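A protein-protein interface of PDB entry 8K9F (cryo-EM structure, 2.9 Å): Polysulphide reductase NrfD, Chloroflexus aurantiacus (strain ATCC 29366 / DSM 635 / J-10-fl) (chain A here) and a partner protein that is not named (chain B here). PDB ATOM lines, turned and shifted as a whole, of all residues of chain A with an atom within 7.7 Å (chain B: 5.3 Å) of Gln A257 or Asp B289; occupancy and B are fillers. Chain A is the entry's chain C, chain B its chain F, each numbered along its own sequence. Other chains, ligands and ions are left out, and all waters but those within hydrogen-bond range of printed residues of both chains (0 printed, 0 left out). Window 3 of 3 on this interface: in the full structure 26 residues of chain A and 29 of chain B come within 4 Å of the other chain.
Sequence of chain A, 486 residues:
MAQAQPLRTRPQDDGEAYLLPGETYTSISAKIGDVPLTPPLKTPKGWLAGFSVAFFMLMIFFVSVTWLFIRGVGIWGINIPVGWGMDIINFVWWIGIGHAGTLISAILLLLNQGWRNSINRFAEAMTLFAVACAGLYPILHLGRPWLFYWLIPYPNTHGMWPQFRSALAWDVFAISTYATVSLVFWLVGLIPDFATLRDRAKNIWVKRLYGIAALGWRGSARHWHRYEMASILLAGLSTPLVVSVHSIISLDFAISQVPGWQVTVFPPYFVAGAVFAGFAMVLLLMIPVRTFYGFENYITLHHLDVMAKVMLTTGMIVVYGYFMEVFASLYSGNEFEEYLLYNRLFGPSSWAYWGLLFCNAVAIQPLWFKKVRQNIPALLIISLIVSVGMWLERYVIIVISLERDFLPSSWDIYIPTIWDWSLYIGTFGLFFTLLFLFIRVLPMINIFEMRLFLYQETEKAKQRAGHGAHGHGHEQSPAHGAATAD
The backbone carbonyl oxygen of Ile A255 lies close to the backbone NH of Gly B288 (3.5 Å). N of Asp B289 sits close to NE2 of Gln A257 (3.4 Å). O of Gly B288 is in hydrogen-bond range of NE2 of Gln A262.
O of Ser A256 lies close to OE1 of Gln A262 (2.9 Å).
CB of Ile A255 touches CB of Ser B287 (3.7 Å). Gln A262 touches Ile B285 (NE2 to CA, 3.7 Å).
Of the printed residues of chain B, Ile A255 touches Ser B287 (3.7 Å) and Gly B288 (3.4 Å). Of chain B, only Asp B289 (3.4 Å) comes within 4 Å of Gln A257. Printed residues of chain B within 4 Å of Gln A262: Ile B285 and Gly B288. Of the printed residues of chain A, Ile B285 touches Gln A262. Printed residues of chain A within 4 Å of Ser B287: Ile A255 (3.7 Å). Of chain A, only Gln A257 comes within 4 Å of Asp B289. The nearest residue of chain A that does not touch Asp B289 is Gln A262 (5.1 Å). The nearest printed residue of chain B that does not touch Gln A262 is Val B290 (4.4 Å).
Of the 14 printed residues of chain A, 3 touch a printed residue of chain B. Among the printed residues, no Asp or Glu carboxylate lies within 4 Å of a Lys or Arg side-chain nitrogen of the other chain.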
ATOM      1  N   ASP A 252     -17.149  34.628  24.191  1.00  0.00           N
ATOM      2  CA  ASP A 252     -16.581  33.977  23.011  1.00  0.00           C
ATOM      3  C   ASP A 252     -16.299  32.492  23.224  1.00  0.00           C
ATOM      4  O   ASP A 252     -15.912  31.812  22.274  1.00  0.00           O
ATOM      5  CB  ASP A 252     -15.337  34.712  22.497  1.00  0.00           C
ATOM      6  CG  ASP A 252     -14.286  34.929  23.553  1.00  0.00           C
ATOM      7  OD1 ASP A 252     -13.780  33.940  24.120  1.00  0.00           O
ATOM      8  OD2 ASP A 252     -13.931  36.102  23.796  1.00  0.00           O
ATOM      9  N   PHE A 253     -16.464  31.976  24.434  1.00  0.00           N
ATOM     10  CA  PHE A 253     -16.625  30.548  24.652  1.00  0.00           C
ATOM     11  C   PHE A 253     -18.057  30.193  24.999  1.00  0.00           C
ATOM     12  O   PHE A 253     -18.565  29.154  24.577  1.00  0.00           O
ATOM     13  CB  PHE A 253     -15.688  30.083  25.768  1.00  0.00           C
ATOM     14  CG  PHE A 253     -14.326  30.689  25.685  1.00  0.00           C
ATOM     15  CD1 PHE A 253     -13.494  30.391  24.623  1.00  0.00           C
ATOM     16  CD2 PHE A 253     -13.897  31.592  26.638  1.00  0.00           C
ATOM     17  CE1 PHE A 253     -12.243  30.966  24.526  1.00  0.00           C
ATOM     18  CE2 PHE A 253     -12.650  32.167  26.552  1.00  0.00           C
ATOM     19  CZ  PHE A 253     -11.821  31.856  25.492  1.00  0.00           C
ATOM     20  N   ALA A 254     -18.733  31.080  25.710  1.00  0.00           N
ATOM     21  CA  ALA A 254     -20.021  30.768  26.296  1.00  0.00           C
ATOM     22  C   ALA A 254     -21.157  30.714  25.279  1.00  0.00           C
ATOM     23  O   ALA A 254     -22.187  30.100  25.566  1.00  0.00           O
ATOM     24  CB  ALA A 254     -20.312  31.786  27.392  1.00  0.00           C
ATOM     25  N   ILE A 255     -21.006  31.331  24.107  1.00  0.00           N
ATOM     26  CA  ILE A 255     -21.990  31.138  23.047  1.00  0.00           C
ATOM     27  C   ILE A 255     -21.644  29.952  22.162  1.00  0.00           C
ATOM     28  O   ILE A 255     -22.480  29.526  21.355  1.00  0.00           O
ATOM     29  CB  ILE A 255     -22.151  32.383  22.155  1.00  0.00           C
ATOM     30  CG1 ILE A 255     -20.942  32.557  21.235  1.00  0.00           C
ATOM     31  CG2 ILE A 255     -22.402  33.610  22.989  1.00  0.00           C
ATOM     32  CD1 ILE A 255     -21.237  33.308  19.960  1.00  0.00           C
ATOM     33  N   SER A 256     -20.443  29.411  22.284  1.00  0.00           N
ATOM     34  CA  SER A 256     -20.034  28.310  21.439  1.00  0.00           C
ATOM     35  C   SER A 256     -20.612  26.994  21.948  1.00  0.00           C
ATOM     36  O   SER A 256     -20.874  26.824  23.135  1.00  0.00           O
ATOM     37  CB  SER A 256     -18.521  28.213  21.391  1.00  0.00           C
ATOM     38  OG  SER A 256     -18.109  27.271  22.353  1.00  0.00           O
ATOM     39  N   GLN A 257     -20.759  26.037  21.035  1.00  0.00           N
ATOM     40  CA  GLN A 257     -21.453  24.785  21.315  1.00  0.00           C
ATOM     41  C   GLN A 257     -20.531  23.677  21.815  1.00  0.00           C
ATOM     42  O   GLN A 257     -20.972  22.530  21.919  1.00  0.00           O
ATOM     43  CB  GLN A 257     -22.215  24.318  20.071  1.00  0.00           C
ATOM     44  CG  GLN A 257     -23.055  25.405  19.414  1.00  0.00           C
ATOM     45  CD  GLN A 257     -24.211  24.861  18.589  1.00  0.00           C
ATOM     46  OE1 GLN A 257     -24.281  23.671  18.306  1.00  0.00           O
ATOM     47  NE2 GLN A 257     -25.128  25.742  18.200  1.00  0.00           N
ATOM     48  N   VAL A 258     -19.276  23.989  22.122  1.00  0.00           N
ATOM     49  CA  VAL A 258     -18.349  23.034  22.748  1.00  0.00           C
ATOM     50  C   VAL A 258     -18.854  22.701  24.150  1.00  0.00           C
ATOM     51  O   VAL A 258     -19.402  23.593  24.820  1.00  0.00           O
ATOM     52  CB  VAL A 258     -16.937  23.637  22.792  1.00  0.00           C
ATOM     53  CG1 VAL A 258     -15.869  22.581  22.958  1.00  0.00           C
ATOM     54  CG2 VAL A 258     -16.669  24.447  21.540  1.00  0.00           C
ATOM     55  N   PRO A 259     -18.760  21.438  24.608  1.00  0.00           N
ATOM     56  CA  PRO A 259     -19.311  21.084  25.933  1.00  0.00           C
ATOM     57  C   PRO A 259     -18.694  21.815  27.116  1.00  0.00           C
ATOM     58  O   PRO A 259     -19.418  22.174  28.052  1.00  0.00           O
ATOM     59  CB  PRO A 259     -19.046  19.576  26.017  1.00  0.00           C
ATOM     60  CG  PRO A 259     -19.079  19.125  24.635  1.00  0.00           C
ATOM     61  CD  PRO A 259     -18.458  20.226  23.824  1.00  0.00           C
ATOM     62  N   GLY A 260     -17.385  22.063  27.100  1.00  0.00           N
ATOM     63  CA  GLY A 260     -16.777  22.794  28.197  1.00  0.00           C
ATOM     64  C   GLY A 260     -16.869  24.288  28.074  1.00  0.00           C
ATOM     65  O   GLY A 260     -16.442  25.005  28.983  1.00  0.00           O
ATOM     66  N   TRP A 261     -17.412  24.770  26.972  1.00  0.00           N
ATOM     67  CA  TRP A 261     -17.490  26.191  26.715  1.00  0.00           C
ATOM     68  C   TRP A 261     -18.899  26.728  26.885  1.00  0.00           C
ATOM     69  O   TRP A 261     -19.076  27.821  27.423  1.00  0.00           O
ATOM     70  CB  TRP A 261     -16.971  26.488  25.307  1.00  0.00           C
ATOM     71  CG  TRP A 261     -15.492  26.357  25.141  1.00  0.00           C
ATOM     72  CD1 TRP A 261     -14.617  25.782  26.007  1.00  0.00           C
ATOM     73  CD2 TRP A 261     -14.715  26.819  24.035  1.00  0.00           C
ATOM     74  NE1 TRP A 261     -13.343  25.847  25.507  1.00  0.00           N
ATOM     75  CE2 TRP A 261     -13.378  26.482  24.296  1.00  0.00           C
ATOM     76  CE3 TRP A 261     -15.021  27.486  22.849  1.00  0.00           C
ATOM     77  CZ2 TRP A 261     -12.351  26.791  23.421  1.00  0.00           C
ATOM     78  CZ3 TRP A 261     -14.006  27.784  21.979  1.00  0.00           C
ATOM     79  CH2 TRP A 261     -12.685  27.441  22.268  1.00  0.00           C
ATOM     80  N   GLN A 262     -19.910  25.972  26.469  1.00  0.00           N
ATOM     81  CA  GLN A 262     -21.300  26.329  26.736  1.00  0.00           C
ATOM     82  C   GLN A 262     -21.573  26.007  28.197  1.00  0.00           C
ATOM     83  O   GLN A 262     -22.022  24.917  28.553  1.00  0.00           O
ATOM     84  CB  GLN A 262     -22.249  25.587  25.801  1.00  0.00           C
ATOM     85  CG  GLN A 262     -23.715  25.911  26.014  1.00  0.00           C
ATOM     86  CD  GLN A 262     -24.275  26.786  24.930  1.00  0.00           C
ATOM     87  OE1 GLN A 262     -23.633  27.007  23.910  1.00  0.00           O
ATOM     88  NE2 GLN A 262     -25.480  27.297  25.146  1.00  0.00           N
ATOM     89  N   SER A 401     -11.032  21.524  26.490  1.00  0.00           N
ATOM     90  CA  SER A 401     -12.334  21.333  25.866  1.00  0.00           C
ATOM     91  C   SER A 401     -12.243  21.282  24.350  1.00  0.00           C
ATOM     92  O   SER A 401     -13.090  20.656  23.707  1.00  0.00           O
ATOM     93  CB  SER A 401     -13.298  22.431  26.281  1.00  0.00           C
ATOM     94  OG  SER A 401     -14.607  22.018  25.971  1.00  0.00           O
ATOM     95  N   ASP A 405     -13.816  16.381  21.588  1.00  0.00           N
ATOM     96  CA  ASP A 405     -15.078  16.936  21.132  1.00  0.00           C
ATOM     97  C   ASP A 405     -16.047  15.806  20.844  1.00  0.00           C
ATOM     98  O   ASP A 405     -15.858  14.681  21.319  1.00  0.00           O
ATOM     99  CB  ASP A 405     -14.876  17.792  19.883  1.00  0.00           C
ATOM    100  CG  ASP A 405     -13.907  18.931  20.107  1.00  0.00           C
ATOM    101  OD1 ASP A 405     -14.252  19.861  20.862  1.00  0.00           O
ATOM    102  OD2 ASP A 405     -12.799  18.893  19.534  1.00  0.00           O
ATOM    103  N   PHE A 406     -17.110  16.126  20.109  1.00  0.00           N
ATOM    104  CA  PHE A 406     -18.205  15.188  19.888  1.00  0.00           C
ATOM    105  C   PHE A 406     -17.769  13.963  19.098  1.00  0.00           C
ATOM    106  O   PHE A 406     -18.142  12.837  19.439  1.00  0.00           O
ATOM    107  CB  PHE A 406     -19.340  15.901  19.166  1.00  0.00           C
ATOM    108  CG  PHE A 406     -19.778  17.161  19.830  1.00  0.00           C
ATOM    109  CD1 PHE A 406     -20.671  17.126  20.882  1.00  0.00           C
ATOM    110  CD2 PHE A 406     -19.312  18.386  19.392  1.00  0.00           C
ATOM    111  CE1 PHE A 406     -21.081  18.283  21.492  1.00  0.00           C
ATOM    112  CE2 PHE A 406     -19.718  19.547  20.003  1.00  0.00           C
ATOM    113  CZ  PHE A 406     -20.608  19.491  21.050  1.00  0.00           C
ATOM    114  N   ILE B 285     -27.698  30.329  26.195  1.00  0.00           N
ATOM    115  CA  ILE B 285     -28.548  29.244  25.731  1.00  0.00           C
ATOM    116  C   ILE B 285     -29.095  29.547  24.338  1.00  0.00           C
ATOM    117  O   ILE B 285     -29.193  28.658  23.482  1.00  0.00           O
ATOM    118  CB  ILE B 285     -29.649  28.993  26.777  1.00  0.00           C
ATOM    119  CG1 ILE B 285     -29.011  28.380  28.025  1.00  0.00           C
ATOM    120  CG2 ILE B 285     -30.726  28.100  26.241  1.00  0.00           C
ATOM    121  CD1 ILE B 285     -29.905  28.296  29.228  1.00  0.00           C
ATOM    122  N   TRP B 286     -29.392  30.817  24.065  1.00  0.00           N
ATOM    123  CA  TRP B 286     -29.989  31.213  22.798  1.00  0.00           C
ATOM    124  C   TRP B 286     -28.985  31.149  21.661  1.00  0.00           C
ATOM    125  O   TRP B 286     -29.300  30.654  20.577  1.00  0.00           O
ATOM    126  CB  TRP B 286     -30.569  32.620  22.936  1.00  0.00           C
ATOM    127  CG  TRP B 286     -31.319  33.108  21.747  1.00  0.00           C
ATOM    128  CD1 TRP B 286     -32.646  32.969  21.507  1.00  0.00           C
ATOM    129  CD2 TRP B 286     -30.786  33.851  20.648  1.00  0.00           C
ATOM    130  NE1 TRP B 286     -32.977  33.565  20.320  1.00  0.00           N
ATOM    131  CE2 TRP B 286     -31.849  34.113  19.770  1.00  0.00           C
ATOM    132  CE3 TRP B 286     -29.510  34.308  20.316  1.00  0.00           C
ATOM    133  CZ2 TRP B 286     -31.679  34.814  18.583  1.00  0.00           C
ATOM    134  CZ3 TRP B 286     -29.342  35.004  19.140  1.00  0.00           C
ATOM    135  CH2 TRP B 286     -30.419  35.251  18.287  1.00  0.00           C
ATOM    136  N   SER B 287     -27.767  31.650  21.882  1.00  0.00           N
ATOM    137  CA  SER B 287     -26.783  31.632  20.808  1.00  0.00           C
ATOM    138  C   SER B 287     -26.232  30.230  20.580  1.00  0.00           C
ATOM    139  O   SER B 287     -26.093  29.794  19.434  1.00  0.00           O
ATOM    140  CB  SER B 287     -25.665  32.619  21.107  1.00  0.00           C
ATOM    141  OG  SER B 287     -26.093  33.946  20.866  1.00  0.00           O
ATOM    142  N   GLY B 288     -25.925  29.503  21.647  1.00  0.00           N
ATOM    143  CA  GLY B 288     -25.556  28.113  21.471  1.00  0.00           C
ATOM    144  C   GLY B 288     -26.774  27.225  21.566  1.00  0.00           C
ATOM    145  O   GLY B 288     -27.158  26.788  22.653  1.00  0.00           O
ATOM    146  N   ASP B 289     -27.367  26.920  20.415  1.00  0.00           N
ATOM    147  CA  ASP B 289     -28.712  26.352  20.340  1.00  0.00           C
ATOM    148  C   ASP B 289     -28.636  24.837  20.488  1.00  0.00           C
ATOM    149  O   ASP B 289     -28.830  24.073  19.541  1.00  0.00           O
ATOM    150  CB  ASP B 289     -29.367  26.755  19.028  1.00  0.00           C
ATOM    151  CG  ASP B 289     -30.863  26.699  19.090  1.00  0.00           C
ATOM    152  OD1 ASP B 289     -31.446  27.494  19.845  1.00  0.00           O
ATOM    153  OD2 ASP B 289     -31.457  25.872  18.371  1.00  0.00           O
ATOM    154  N   VAL B 290     -28.352  24.397  21.707  1.00  0.00           N
ATOM    155  CA  VAL B 290     -28.172  22.984  22.009  1.00  0.00           C
ATOM    156  C   VAL B 290     -29.404  22.517  22.772  1.00  0.00           C
ATOM    157  O   VAL B 290     -29.852  23.186  23.711  1.00  0.00           O
ATOM    158  CB  VAL B 290     -26.880  22.747  22.809  1.00  0.00           C
ATOM    159  CG1 VAL B 290     -26.515  21.293  22.787  1.00  0.00           C
ATOM    160  CG2 VAL B 290     -25.751  23.569  22.250  1.00  0.00           C
ATOM    161  N   ALA B 291     -29.950  21.370  22.378  1.00  0.00           N
ATOM    162  CA  ALA B 291     -31.332  21.029  22.698  1.00  0.00           C
ATOM    163  C   ALA B 291     -31.541  20.443  24.093  1.00  0.00           C
ATOM    164  O   ALA B 291     -32.624  19.916  24.360  1.00  0.00           O
ATOM    165  CB  ALA B 291     -31.892  20.058  21.659  1.00  0.00           C
ATOM    166  N   THR B 294     -32.250  24.492  25.604  1.00  0.00           N
ATOM    167  CA  THR B 294     -33.278  25.210  24.860  1.00  0.00           C
ATOM    168  C   THR B 294     -34.733  24.961  25.314  1.00  0.00           C
ATOM    169  O   THR B 294     -35.510  25.928  25.283  1.00  0.00           O
ATOM    170  CB  THR B 294     -33.046  24.903  23.367  1.00  0.00           C
ATOM    171  OG1 THR B 294     -31.857  25.569  22.932  1.00  0.00           O
ATOM    172  CG2 THR B 294     -34.175  25.349  22.491  1.00  0.00           C
